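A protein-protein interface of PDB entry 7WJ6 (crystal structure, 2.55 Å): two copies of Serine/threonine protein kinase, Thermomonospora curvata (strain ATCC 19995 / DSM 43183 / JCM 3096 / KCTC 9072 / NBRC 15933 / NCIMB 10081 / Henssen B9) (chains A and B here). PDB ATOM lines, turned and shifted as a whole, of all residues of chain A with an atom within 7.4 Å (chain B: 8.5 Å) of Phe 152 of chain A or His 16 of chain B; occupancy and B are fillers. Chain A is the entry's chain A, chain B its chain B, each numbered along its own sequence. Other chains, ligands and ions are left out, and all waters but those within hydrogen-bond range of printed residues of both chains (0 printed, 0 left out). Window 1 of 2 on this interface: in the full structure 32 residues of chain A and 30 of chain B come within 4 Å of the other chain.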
ATOM      1  N   ALA A  97     -23.708  10.028   0.294  1.00  0.00           N
ATOM      2  CA  ALA A  97     -22.365   9.780  -0.203  1.00  0.00           C
ATOM      3  C   ALA A  97     -22.049   8.289  -0.149  1.00  0.00           C
ATOM      4  O   ALA A  97     -22.441   7.591   0.789  1.00  0.00           O
ATOM      5  CB  ALA A  97     -21.346  10.572   0.613  1.00  0.00           C
ATOM      6  N   LEU A  98     -21.329   7.804  -1.165  1.00  0.00           N
ATOM      7  CA  LEU A  98     -21.074   6.372  -1.290  1.00  0.00           C
ATOM      8  C   LEU A  98     -20.295   5.820  -0.101  1.00  0.00           C
ATOM      9  O   LEU A  98     -20.460   4.648   0.260  1.00  0.00           O
ATOM     10  CB  LEU A  98     -20.327   6.091  -2.599  1.00  0.00           C
ATOM     11  CG  LEU A  98     -20.127   4.631  -3.020  1.00  0.00           C
ATOM     12  CD1 LEU A  98     -21.457   3.943  -3.270  1.00  0.00           C
ATOM     13  CD2 LEU A  98     -19.245   4.544  -4.249  1.00  0.00           C
ATOM     14  N   ASN A  99     -19.448   6.640   0.524  1.00  0.00           N
ATOM     15  CA  ASN A  99     -18.661   6.173   1.659  1.00  0.00           C
ATOM     16  C   ASN A  99     -19.519   5.862   2.880  1.00  0.00           C
ATOM     17  O   ASN A  99     -19.077   5.106   3.753  1.00  0.00           O
ATOM     18  CB  ASN A  99     -17.587   7.204   2.023  1.00  0.00           C
ATOM     19  CG  ASN A  99     -18.172   8.494   2.577  1.00  0.00           C
ATOM     20  OD1 ASN A  99     -18.630   9.357   1.825  1.00  0.00           O
ATOM     21  ND2 ASN A  99     -18.148   8.635   3.898  1.00  0.00           N
ATOM     22  N   THR A 100     -20.724   6.430   2.972  1.00  0.00           N
ATOM     23  CA  THR A 100     -21.595   6.170   4.112  1.00  0.00           C
ATOM     24  C   THR A 100     -22.286   4.815   4.044  1.00  0.00           C
ATOM     25  O   THR A 100     -22.868   4.385   5.046  1.00  0.00           O
ATOM     26  CB  THR A 100     -22.653   7.269   4.237  1.00  0.00           C
ATOM     27  OG1 THR A 100     -23.611   7.137   3.180  1.00  0.00           O
ATOM     28  CG2 THR A 100     -22.005   8.642   4.160  1.00  0.00           C
ATOM     29  N   TYR A 146     -11.308  14.421 -13.915  1.00  0.00           N
ATOM     30  CA  TYR A 146     -11.860  14.616 -12.576  1.00  0.00           C
ATOM     31  C   TYR A 146     -10.809  14.485 -11.475  1.00  0.00           C
ATOM     32  O   TYR A 146     -10.919  15.161 -10.445  1.00  0.00           O
ATOM     33  CB  TYR A 146     -13.007  13.633 -12.316  1.00  0.00           C
ATOM     34  CG  TYR A 146     -13.724  13.908 -11.010  1.00  0.00           C
ATOM     35  CD1 TYR A 146     -14.615  14.967 -10.896  1.00  0.00           C
ATOM     36  CD2 TYR A 146     -13.496  13.122  -9.889  1.00  0.00           C
ATOM     37  CE1 TYR A 146     -15.264  15.233  -9.707  1.00  0.00           C
ATOM     38  CE2 TYR A 146     -14.139  13.379  -8.697  1.00  0.00           C
ATOM     39  CZ  TYR A 146     -15.021  14.435  -8.612  1.00  0.00           C
ATOM     40  OH  TYR A 146     -15.664  14.692  -7.426  1.00  0.00           O
ATOM     41  N   ASP A 148      -9.975  13.182  -8.795  1.00  0.00           N
ATOM     42  CA  ASP A 148     -10.181  12.834  -7.395  1.00  0.00           C
ATOM     43  C   ASP A 148     -11.349  11.870  -7.219  1.00  0.00           C
ATOM     44  O   ASP A 148     -12.088  11.932  -6.232  1.00  0.00           O
ATOM     45  CB  ASP A 148     -10.396  14.092  -6.556  1.00  0.00           C
ATOM     46  CG  ASP A 148      -9.855  13.957  -5.149  1.00  0.00           C
ATOM     47  OD1 ASP A 148      -8.999  13.073  -4.919  1.00  0.00           O
ATOM     48  OD2 ASP A 148     -10.286  14.735  -4.272  1.00  0.00           O
ATOM     49  N   LEU A 149     -11.528  10.955  -8.165  1.00  0.00           N
ATOM     50  CA  LEU A 149     -12.691  10.078  -8.145  1.00  0.00           C
ATOM     51  C   LEU A 149     -12.485   8.978  -7.112  1.00  0.00           C
ATOM     52  O   LEU A 149     -11.544   8.185  -7.220  1.00  0.00           O
ATOM     53  CB  LEU A 149     -12.935   9.479  -9.528  1.00  0.00           C
ATOM     54  CG  LEU A 149     -14.084   8.472  -9.572  1.00  0.00           C
ATOM     55  CD1 LEU A 149     -15.427   9.178  -9.496  1.00  0.00           C
ATOM     56  CD2 LEU A 149     -13.993   7.637 -10.821  1.00  0.00           C
ATOM     57  N   HIS A 150     -13.364   8.931  -6.117  1.00  0.00           N
ATOM     58  CA  HIS A 150     -13.355   7.882  -5.102  1.00  0.00           C
ATOM     59  C   HIS A 150     -14.686   7.946  -4.359  1.00  0.00           C
ATOM     60  O   HIS A 150     -15.551   8.772  -4.667  1.00  0.00           O
ATOM     61  CB  HIS A 150     -12.159   8.017  -4.154  1.00  0.00           C
ATOM     62  CG  HIS A 150     -11.972   9.393  -3.597  1.00  0.00           C
ATOM     63  ND1 HIS A 150     -12.871   9.978  -2.730  1.00  0.00           N
ATOM     64  CD2 HIS A 150     -10.982  10.300  -3.780  1.00  0.00           C
ATOM     65  CE1 HIS A 150     -12.445  11.186  -2.406  1.00  0.00           C
ATOM     66  NE2 HIS A 150     -11.302  11.406  -3.031  1.00  0.00           N
ATOM     67  N   MET A 151     -14.834   7.079  -3.353  1.00  0.00           N
ATOM     68  CA  MET A 151     -16.142   6.879  -2.735  1.00  0.00           C
ATOM     69  C   MET A 151     -16.614   8.084  -1.930  1.00  0.00           C
ATOM     70  O   MET A 151     -17.812   8.187  -1.647  1.00  0.00           O
ATOM     71  CB  MET A 151     -16.129   5.631  -1.847  1.00  0.00           C
ATOM     72  CG  MET A 151     -15.346   5.761  -0.550  1.00  0.00           C
ATOM     73  SD  MET A 151     -15.186   4.170   0.293  1.00  0.00           S
ATOM     74  CE  MET A 151     -13.612   4.386   1.116  1.00  0.00           C
ATOM     75  N   PHE A 152     -15.712   8.991  -1.547  1.00  0.00           N
ATOM     76  CA  PHE A 152     -16.133  10.166  -0.790  1.00  0.00           C
ATOM     77  C   PHE A 152     -16.695  11.270  -1.681  1.00  0.00           C
ATOM     78  O   PHE A 152     -17.369  12.171  -1.175  1.00  0.00           O
ATOM     79  CB  PHE A 152     -14.968  10.717   0.036  1.00  0.00           C
ATOM     80  CG  PHE A 152     -14.473   9.777   1.103  1.00  0.00           C
ATOM     81  CD1 PHE A 152     -13.468   8.860   0.828  1.00  0.00           C
ATOM     82  CD2 PHE A 152     -15.003   9.815   2.387  1.00  0.00           C
ATOM     83  CE1 PHE A 152     -13.000   7.994   1.813  1.00  0.00           C
ATOM     84  CE2 PHE A 152     -14.539   8.950   3.376  1.00  0.00           C
ATOM     85  CZ  PHE A 152     -13.535   8.039   3.086  1.00  0.00           C
ATOM     86  N   ASN A 153     -16.441  11.216  -2.987  1.00  0.00           N
ATOM     87  CA  ASN A 153     -16.912  12.229  -3.922  1.00  0.00           C
ATOM     88  C   ASN A 153     -18.158  11.806  -4.686  1.00  0.00           C
ATOM     89  O   ASN A 153     -18.670  12.592  -5.489  1.00  0.00           O
ATOM     90  CB  ASN A 153     -15.805  12.581  -4.917  1.00  0.00           C
ATOM     91  CG  ASN A 153     -14.824  13.585  -4.361  1.00  0.00           C
ATOM     92  OD1 ASN A 153     -15.213  14.550  -3.704  1.00  0.00           O
ATOM     93  ND2 ASN A 153     -13.541  13.361  -4.620  1.00  0.00           N
ATOM     94  N   ILE A 154     -18.648  10.588  -4.474  1.00  0.00           N
ATOM     95  CA  ILE A 154     -19.754  10.040  -5.250  1.00  0.00           C
ATOM     96  C   ILE A 154     -21.033  10.108  -4.426  1.00  0.00           C
ATOM     97  O   ILE A 154     -21.084   9.601  -3.298  1.00  0.00           O
ATOM     98  CB  ILE A 154     -19.460   8.598  -5.693  1.00  0.00           C
ATOM     99  CG1 ILE A 154     -18.256   8.566  -6.633  1.00  0.00           C
ATOM    100  CG2 ILE A 154     -20.677   7.986  -6.368  1.00  0.00           C
ATOM    101  CD1 ILE A 154     -17.812   7.170  -6.990  1.00  0.00           C
ATOM    102  N   MET A 155     -22.065  10.721  -4.996  1.00  0.00           N
ATOM    103  CA  MET A 155     -23.383  10.807  -4.382  1.00  0.00           C
ATOM    104  C   MET A 155     -24.316   9.812  -5.055  1.00  0.00           C
ATOM    105  O   MET A 155     -24.360   9.735  -6.287  1.00  0.00           O
ATOM    106  CB  MET A 155     -23.963  12.217  -4.514  1.00  0.00           C
ATOM    107  CG  MET A 155     -23.399  13.235  -3.547  1.00  0.00           C
ATOM    108  SD  MET A 155     -23.858  12.913  -1.843  1.00  0.00           S
ATOM    109  CE  MET A 155     -25.347  13.899  -1.694  1.00  0.00           C
ATOM    110  N   ILE A 165     -19.447  15.583  -6.401  1.00  0.00           N
ATOM    111  CA  ILE A 165     -19.671  16.754  -5.561  1.00  0.00           C
ATOM    112  C   ILE A 165     -18.548  17.773  -5.690  1.00  0.00           C
ATOM    113  O   ILE A 165     -18.801  18.952  -5.945  1.00  0.00           O
ATOM    114  CB  ILE A 165     -19.897  16.359  -4.086  1.00  0.00           C
ATOM    115  CG1 ILE A 165     -19.017  15.180  -3.689  1.00  0.00           C
ATOM    116  CG2 ILE A 165     -21.364  16.077  -3.841  1.00  0.00           C
ATOM    117  CD1 ILE A 165     -19.205  14.749  -2.255  1.00  0.00           C
ATOM    118  N   ASP A 166     -17.304  17.348  -5.510  1.00  0.00           N
ATOM    119  CA  ASP A 166     -16.189  18.279  -5.384  1.00  0.00           C
ATOM    120  C   ASP A 166     -15.392  18.311  -6.681  1.00  0.00           C
ATOM    121  O   ASP A 166     -14.858  17.285  -7.114  1.00  0.00           O
ATOM    122  CB  ASP A 166     -15.290  17.888  -4.211  1.00  0.00           C
ATOM    123  CG  ASP A 166     -14.386  19.019  -3.770  1.00  0.00           C
ATOM    124  OD1 ASP A 166     -13.549  18.794  -2.871  1.00  0.00           O
ATOM    125  OD2 ASP A 166     -14.515  20.134  -4.320  1.00  0.00           O
ATOM    126  N   PRO A 184      -7.902   6.435  -1.941  1.00  0.00           N
ATOM    127  CA  PRO A 184      -8.048   5.900  -0.576  1.00  0.00           C
ATOM    128  C   PRO A 184      -7.714   4.424  -0.451  1.00  0.00           C
ATOM    129  O   PRO A 184      -7.336   3.978   0.638  1.00  0.00           O
ATOM    130  CB  PRO A 184      -9.528   6.162  -0.253  1.00  0.00           C
ATOM    131  CG  PRO A 184      -9.932   7.263  -1.159  1.00  0.00           C
ATOM    132  CD  PRO A 184      -9.129   7.095  -2.413  1.00  0.00           C
ATOM    133  N   LEU A 205     -12.128   1.609  -7.803  1.00  0.00           N
ATOM    134  CA  LEU A 205     -13.488   1.631  -7.283  1.00  0.00           C
ATOM    135  C   LEU A 205     -14.171   0.278  -7.454  1.00  0.00           C
ATOM    136  O   LEU A 205     -14.986  -0.111  -6.608  1.00  0.00           O
ATOM    137  CB  LEU A 205     -14.290   2.738  -7.969  1.00  0.00           C
ATOM    138  CG  LEU A 205     -15.738   2.935  -7.523  1.00  0.00           C
ATOM    139  CD1 LEU A 205     -15.794   3.393  -6.071  1.00  0.00           C
ATOM    140  CD2 LEU A 205     -16.450   3.919  -8.439  1.00  0.00           C
ATOM    141  N   LEU A 213     -13.524  -2.771   4.552  1.00  0.00           N
ATOM    142  CA  LEU A 213     -12.728  -1.563   4.752  1.00  0.00           C
ATOM    143  C   LEU A 213     -11.317  -1.881   5.238  1.00  0.00           C
ATOM    144  O   LEU A 213     -10.342  -1.290   4.757  1.00  0.00           O
ATOM    145  CB  LEU A 213     -13.440  -0.627   5.729  1.00  0.00           C
ATOM    146  CG  LEU A 213     -14.195   0.533   5.068  1.00  0.00           C
ATOM    147  CD1 LEU A 213     -14.790   1.467   6.109  1.00  0.00           C
ATOM    148  CD2 LEU A 213     -13.290   1.301   4.109  1.00  0.00           C
ATOM    149  N   ALA B  13     -16.128   2.394   9.664  1.00  0.00           N
ATOM    150  CA  ALA B  13     -16.751   3.496   8.952  1.00  0.00           C
ATOM    151  C   ALA B  13     -15.673   4.366   8.328  1.00  0.00           C
ATOM    152  O   ALA B  13     -14.562   4.481   8.853  1.00  0.00           O
ATOM    153  CB  ALA B  13     -17.637   4.329   9.885  1.00  0.00           C
ATOM    154  N   ALA B  14     -16.012   4.966   7.189  1.00  0.00           N
ATOM    155  CA  ALA B  14     -15.148   5.915   6.498  1.00  0.00           C
ATOM    156  C   ALA B  14     -15.692   7.318   6.722  1.00  0.00           C
ATOM    157  O   ALA B  14     -16.813   7.624   6.305  1.00  0.00           O
ATOM    158  CB  ALA B  14     -15.073   5.594   5.006  1.00  0.00           C
ATOM    159  N   LEU B  15     -14.893   8.173   7.360  1.00  0.00           N
ATOM    160  CA  LEU B  15     -15.382   9.479   7.797  1.00  0.00           C
ATOM    161  C   LEU B  15     -15.123  10.566   6.756  1.00  0.00           C
ATOM    162  O   LEU B  15     -16.058  11.232   6.304  1.00  0.00           O
ATOM    163  CB  LEU B  15     -14.756   9.844   9.147  1.00  0.00           C
ATOM    164  CG  LEU B  15     -15.042   8.822  10.254  1.00  0.00           C
ATOM    165  CD1 LEU B  15     -14.485   9.286  11.589  1.00  0.00           C
ATOM    166  CD2 LEU B  15     -16.538   8.536  10.355  1.00  0.00           C
ATOM    167  N   HIS B  16     -13.863  10.774   6.382  1.00  0.00           N
ATOM    168  CA  HIS B  16     -13.558  11.720   5.318  1.00  0.00           C
ATOM    169  C   HIS B  16     -12.183  11.410   4.757  1.00  0.00           C
ATOM    170  O   HIS B  16     -11.393  10.681   5.362  1.00  0.00           O
ATOM    171  CB  HIS B  16     -13.631  13.179   5.792  1.00  0.00           C
ATOM    172  CG  HIS B  16     -13.294  13.371   7.236  1.00  0.00           C
ATOM    173  ND1 HIS B  16     -14.252  13.397   8.226  1.00  0.00           N
ATOM    174  CD2 HIS B  16     -12.106  13.569   7.856  1.00  0.00           C
ATOM    175  CE1 HIS B  16     -13.669  13.589   9.396  1.00  0.00           C
ATOM    176  NE2 HIS B  16     -12.367  13.696   9.199  1.00  0.00           N
ATOM    177  N   PHE B  17     -11.924  11.965   3.572  1.00  0.00           N
ATOM    178  CA  PHE B  17     -10.672  11.780   2.849  1.00  0.00           C
ATOM    179  C   PHE B  17     -10.343  13.065   2.105  1.00  0.00           C
ATOM    180  O   PHE B  17     -11.221  13.652   1.469  1.00  0.00           O
ATOM    181  CB  PHE B  17     -10.773  10.607   1.868  1.00  0.00           C
ATOM    182  CG  PHE B  17      -9.493  10.304   1.140  1.00  0.00           C
ATOM    183  CD1 PHE B  17      -8.578   9.407   1.663  1.00  0.00           C
ATOM    184  CD2 PHE B  17      -9.215  10.900  -0.076  1.00  0.00           C
ATOM    185  CE1 PHE B  17      -7.407   9.121   0.994  1.00  0.00           C
ATOM    186  CE2 PHE B  17      -8.047  10.616  -0.749  1.00  0.00           C
ATOM    187  CZ  PHE B  17      -7.143   9.725  -0.214  1.00  0.00           C
ATOM    188  N   SER B  18      -9.091  13.505   2.191  1.00  0.00           N
ATOM    189  CA  SER B  18      -8.678  14.704   1.479  1.00  0.00           C
ATOM    190  C   SER B  18      -7.162  14.739   1.378  1.00  0.00           C
ATOM    191  O   SER B  18      -6.463  14.449   2.355  1.00  0.00           O
ATOM    192  CB  SER B  18      -9.180  15.976   2.170  1.00  0.00           C
ATOM    193  OG  SER B  18      -9.183  17.069   1.268  1.00  0.00           O
ATOM    194  N   ASN B  19      -6.671  15.112   0.197  1.00  0.00           N
ATOM    195  CA  ASN B  19      -5.241  15.295  -0.049  1.00  0.00           C
ATOM    196  C   ASN B  19      -4.446  14.051   0.344  1.00  0.00           C
ATOM    197  O   ASN B  19      -3.435  14.120   1.044  1.00  0.00           O
ATOM    198  CB  ASN B  19      -4.721  16.538   0.677  1.00  0.00           C
ATOM    199  N   GLY B  20      -4.926  12.895  -0.110  1.00  0.00           N
ATOM    200  CA  GLY B  20      -4.259  11.641   0.171  1.00  0.00           C
ATOM    201  C   GLY B  20      -4.305  11.191   1.612  1.00  0.00           C
ATOM    202  O   GLY B  20      -3.551  10.288   1.986  1.00  0.00           O
ATOM    203  N   GLY B  21      -5.154  11.797   2.439  1.00  0.00           N
ATOM    204  CA  GLY B  21      -5.265  11.383   3.824  1.00  0.00           C
ATOM    205  C   GLY B  21      -6.687  11.041   4.216  1.00  0.00           C
ATOM    206  O   GLY B  21      -7.603  11.851   4.039  1.00  0.00           O
ATOM    207  N   GLY B  22      -6.883   9.841   4.755  1.00  0.00           N
ATOM    208  CA  GLY B  22      -8.196   9.365   5.150  1.00  0.00           C
ATOM    209  C   GLY B  22      -8.348   9.300   6.656  1.00  0.00           C
ATOM    210  O   GLY B  22      -7.366   9.149   7.386  1.00  0.00           O
ATOM    211  N   VAL B  23      -9.590   9.426   7.120  1.00  0.00           N
ATOM    212  CA  VAL B  23      -9.929   9.318   8.534  1.00  0.00           C
ATOM    213  C   VAL B  23     -11.024   8.272   8.673  1.00  0.00           C
ATOM    214  O   VAL B  23     -12.048   8.347   7.986  1.00  0.00           O
ATOM    215  CB  VAL B  23     -10.388  10.666   9.121  1.00  0.00           C
ATOM    216  CG1 VAL B  23     -10.890  10.478  10.544  1.00  0.00           C
ATOM    217  CG2 VAL B  23      -9.248  11.676   9.079  1.00  0.00           C
ATOM    218  N   TYR B  24     -10.815   7.304   9.563  1.00  0.00           N
ATOM    219  CA  TYR B  24     -11.733   6.185   9.711  1.00  0.00           C
ATOM    220  C   TYR B  24     -11.992   5.910  11.185  1.00  0.00           C
ATOM    221  O   TYR B  24     -11.134   6.143  12.040  1.00  0.00           O
ATOM    222  CB  TYR B  24     -11.188   4.921   9.034  1.00  0.00           C
ATOM    223  CG  TYR B  24     -10.847   5.115   7.576  1.00  0.00           C
ATOM    224  CD1 TYR B  24      -9.599   5.578   7.197  1.00  0.00           C
ATOM    225  CD2 TYR B  24     -11.775   4.840   6.579  1.00  0.00           C
ATOM    226  CE1 TYR B  24      -9.278   5.761   5.868  1.00  0.00           C
ATOM    227  CE2 TYR B  24     -11.463   5.018   5.243  1.00  0.00           C
ATOM    228  CZ  TYR B  24     -10.209   5.480   4.894  1.00  0.00           C
ATOM    229  OH  TYR B  24      -9.874   5.663   3.570  1.00  0.00           O
ATOM    230  N   ALA B  25     -13.194   5.417  11.470  1.00  0.00           N
ATOM    231  CA  ALA B  25     -13.571   4.966  12.802  1.00  0.00           C
ATOM    232  C   ALA B  25     -13.417   3.453  12.881  1.00  0.00           C
ATOM    233  O   ALA B  25     -13.827   2.734  11.966  1.00  0.00           O
ATOM    234  CB  ALA B  25     -15.007   5.372  13.138  1.00  0.00           C
ATOM    235  N   VAL B  36      -9.997   6.036  16.375  1.00  0.00           N
ATOM    236  CA  VAL B  36      -9.977   6.747  15.103  1.00  0.00           C
ATOM    237  C   VAL B  36      -8.656   6.422  14.423  1.00  0.00           C
ATOM    238  O   VAL B  36      -7.600   6.447  15.066  1.00  0.00           O
ATOM    239  CB  VAL B  36     -10.142   8.265  15.293  1.00  0.00           C
ATOM    240  CG1 VAL B  36      -9.845   8.998  13.997  1.00  0.00           C
ATOM    241  CG2 VAL B  36     -11.544   8.590  15.790  1.00  0.00           C
ATOM    242  N   LEU B  37      -8.713   6.088  13.137  1.00  0.00           N
ATOM    243  CA  LEU B  37      -7.527   5.734  12.365  1.00  0.00           C
ATOM    244  C   LEU B  37      -7.322   6.769  11.272  1.00  0.00           C
ATOM    245  O   LEU B  37      -8.216   6.994  10.446  1.00  0.00           O
ATOM    246  CB  LEU B  37      -7.655   4.324  11.774  1.00  0.00           C
ATOM    247  CG  LEU B  37      -6.574   3.754  10.841  1.00  0.00           C
ATOM    248  CD1 LEU B  37      -6.770   4.141   9.374  1.00  0.00           C
ATOM    249  CD2 LEU B  37      -5.194   4.170  11.313  1.00  0.00           C
ATOM    250  N   LYS B  38      -6.154   7.401  11.271  1.00  0.00           N
ATOM    251  CA  LYS B  38      -5.777   8.332  10.219  1.00  0.00           C
ATOM    252  C   LYS B  38      -4.659   7.708   9.400  1.00  0.00           C
ATOM    253  O   LYS B  38      -3.686   7.191   9.960  1.00  0.00           O
ATOM    254  CB  LYS B  38      -5.340   9.679  10.800  1.00  0.00           C
ATOM    255  CG  LYS B  38      -6.471  10.452  11.463  1.00  0.00           C
ATOM    256  CD  LYS B  38      -6.085  11.897  11.731  1.00  0.00           C
ATOM    257  CE  LYS B  38      -7.250  12.668  12.333  1.00  0.00           C
ATOM    258  NZ  LYS B  38      -6.924  14.106  12.529  1.00  0.00           N
ATOM    259  N   GLU B  39      -4.805   7.751   8.079  1.00  0.00           N
ATOM    260  CA  GLU B  39      -3.900   7.074   7.166  1.00  0.00           C
ATOM    261  C   GLU B  39      -3.440   8.063   6.106  1.00  0.00           C
ATOM    262  O   GLU B  39      -4.163   8.995   5.749  1.00  0.00           O
ATOM    263  CB  GLU B  39      -4.555   5.849   6.518  1.00  0.00           C
ATOM    264  CG  GLU B  39      -5.855   6.153   5.818  1.00  0.00           C
ATOM    265  CD  GLU B  39      -5.693   6.234   4.317  1.00  0.00           C
ATOM    266  OE1 GLU B  39      -4.543   6.106   3.834  1.00  0.00           O
ATOM    267  OE2 GLU B  39      -6.716   6.423   3.622  1.00  0.00           O
ATOM    268  N   ARG B  92     -10.960   7.996  20.244  1.00  0.00           N
ATOM    269  CA  ARG B  92     -12.203   8.560  19.738  1.00  0.00           C
ATOM    270  C   ARG B  92     -12.829   9.444  20.811  1.00  0.00           C
ATOM    271  O   ARG B  92     -13.166   8.964  21.898  1.00  0.00           O
ATOM    272  CB  ARG B  92     -13.159   7.439  19.331  1.00  0.00           C
ATOM    273  CG  ARG B  92     -14.372   7.881  18.531  1.00  0.00           C
ATOM    274  CD  ARG B  92     -14.917   6.710  17.723  1.00  0.00           C
ATOM    275  NE  ARG B  92     -16.105   7.060  16.955  1.00  0.00           N
ATOM    276  CZ  ARG B  92     -16.088   7.739  15.816  1.00  0.00           C
ATOM    277  NH1 ARG B  92     -14.957   8.174  15.287  1.00  0.00           N
ATOM    278  NH2 ARG B  92     -17.235   7.981  15.189  1.00  0.00           N
ATOM    279  N   ILE B 165     -10.117  18.578  17.718  1.00  0.00           N
ATOM    280  CA  ILE B 165     -10.055  17.350  16.923  1.00  0.00           C
ATOM    281  C   ILE B 165      -8.786  17.278  16.069  1.00  0.00           C
ATOM    282  O   ILE B 165      -8.028  16.309  16.154  1.00  0.00           O
ATOM    283  CB  ILE B 165     -11.328  17.171  16.064  1.00  0.00           C
ATOM    284  CG1 ILE B 165     -11.564  18.361  15.133  1.00  0.00           C
ATOM    285  CG2 ILE B 165     -12.527  16.996  16.958  1.00  0.00           C
ATOM    286  CD1 ILE B 165     -12.048  17.968  13.750  1.00  0.00           C
ATOM    287  N   ASP B 166      -8.543  18.280  15.235  1.00  0.00           N
ATOM    288  CA  ASP B 166      -7.481  18.207  14.241  1.00  0.00           C
ATOM    289  C   ASP B 166      -6.338  19.115  14.669  1.00  0.00           C
ATOM    290  O   ASP B 166      -6.529  20.325  14.835  1.00  0.00           O
ATOM    291  CB  ASP B 166      -7.997  18.581  12.851  1.00  0.00           C
ATOM    292  CG  ASP B 166      -6.881  18.715  11.831  1.00  0.00           C
ATOM    293  OD1 ASP B 166      -6.520  17.691  11.211  1.00  0.00           O
ATOM    294  OD2 ASP B 166      -6.371  19.839  11.638  1.00  0.00           O
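The backbone carbonyl oxygen of Ala 14 of chain B lies within hydrogen-bond range of the side-chain amide nitrogen of Asn 99 of chain A (2.9 Å).
The backbone carbonyl oxygen of Met 151 of chain A sits at hydrogen-bond distance from the backbone NH of Asn 99 of chain A, 3.1 Å away. O of Asp 148 of chain A sits close to NE2 of His 150 of chain A. N of Ala 25 of chain B sits at hydrogen-bond distance from O of Ala 13 of chain B, at 3.1 Å. O of His 16 of chain B sits at hydrogen-bond distance from N of Val 23 of chain B, 2.8 Å away. The backbone carbonyl oxygen of Gly 22 of chain B is in hydrogen-bond range of the backbone NH of Glu 39 of chain B. The backbone carbonyl oxygen (O) of Tyr 24 of chain B sits at hydrogen-bond distance from the backbone NH (N) of Leu 37 of chain B (2.7 Å).
Among the printed residues, pairs that only touch across the chains: His 150 of chain A with Phe 17 of chain B, Phe 152 of chain A with Ala 14 of chain B, Phe 152 of chain A with Leu 15 of chain B, Phe 152 of chain A with His 16 of chain B, Phe 152 of chain A with Phe 17 of chain B, Pro 184 of chain A with Phe 17 of chain B, Pro 184 of chain A with Tyr 24 of chain B, Pro 184 of chain A with Glu 39 of chain B, Leu 213 of chain A with Ala 13 of chain B and Leu 213 of chain A with Ala 14 of chain B.
Phe 152 of chain A touches four residues of chain B. Printed residues of chain A within 4 Å of His 16 of chain B: Phe 152. Of the printed residues of chain A, Ala 13 of chain B touches Leu 213 (3.8 Å). Printed residues of chain B within 4 Å of Asn 99 of chain A: Ala 14. Ile 165 of chain A touches none of the printed residues of chain B. Leu 205 of chain A touches none of the printed residues of chain B.
Of the 18 printed residues of chain A, 5 touch a printed residue of chain B. Hydrophobic or aromatic side chains of chain B that line the printed part of chain A: Ala 14, Phe 17 and Tyr 24. Along chain B the printed residues that touch a printed residue of chain A span positions 13 to 39.
Positions printed for both chains: 165 and 166. Of the 11 pairs that touch across the chains among the printed residues, none has its exchanged pair printed and touching as well.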
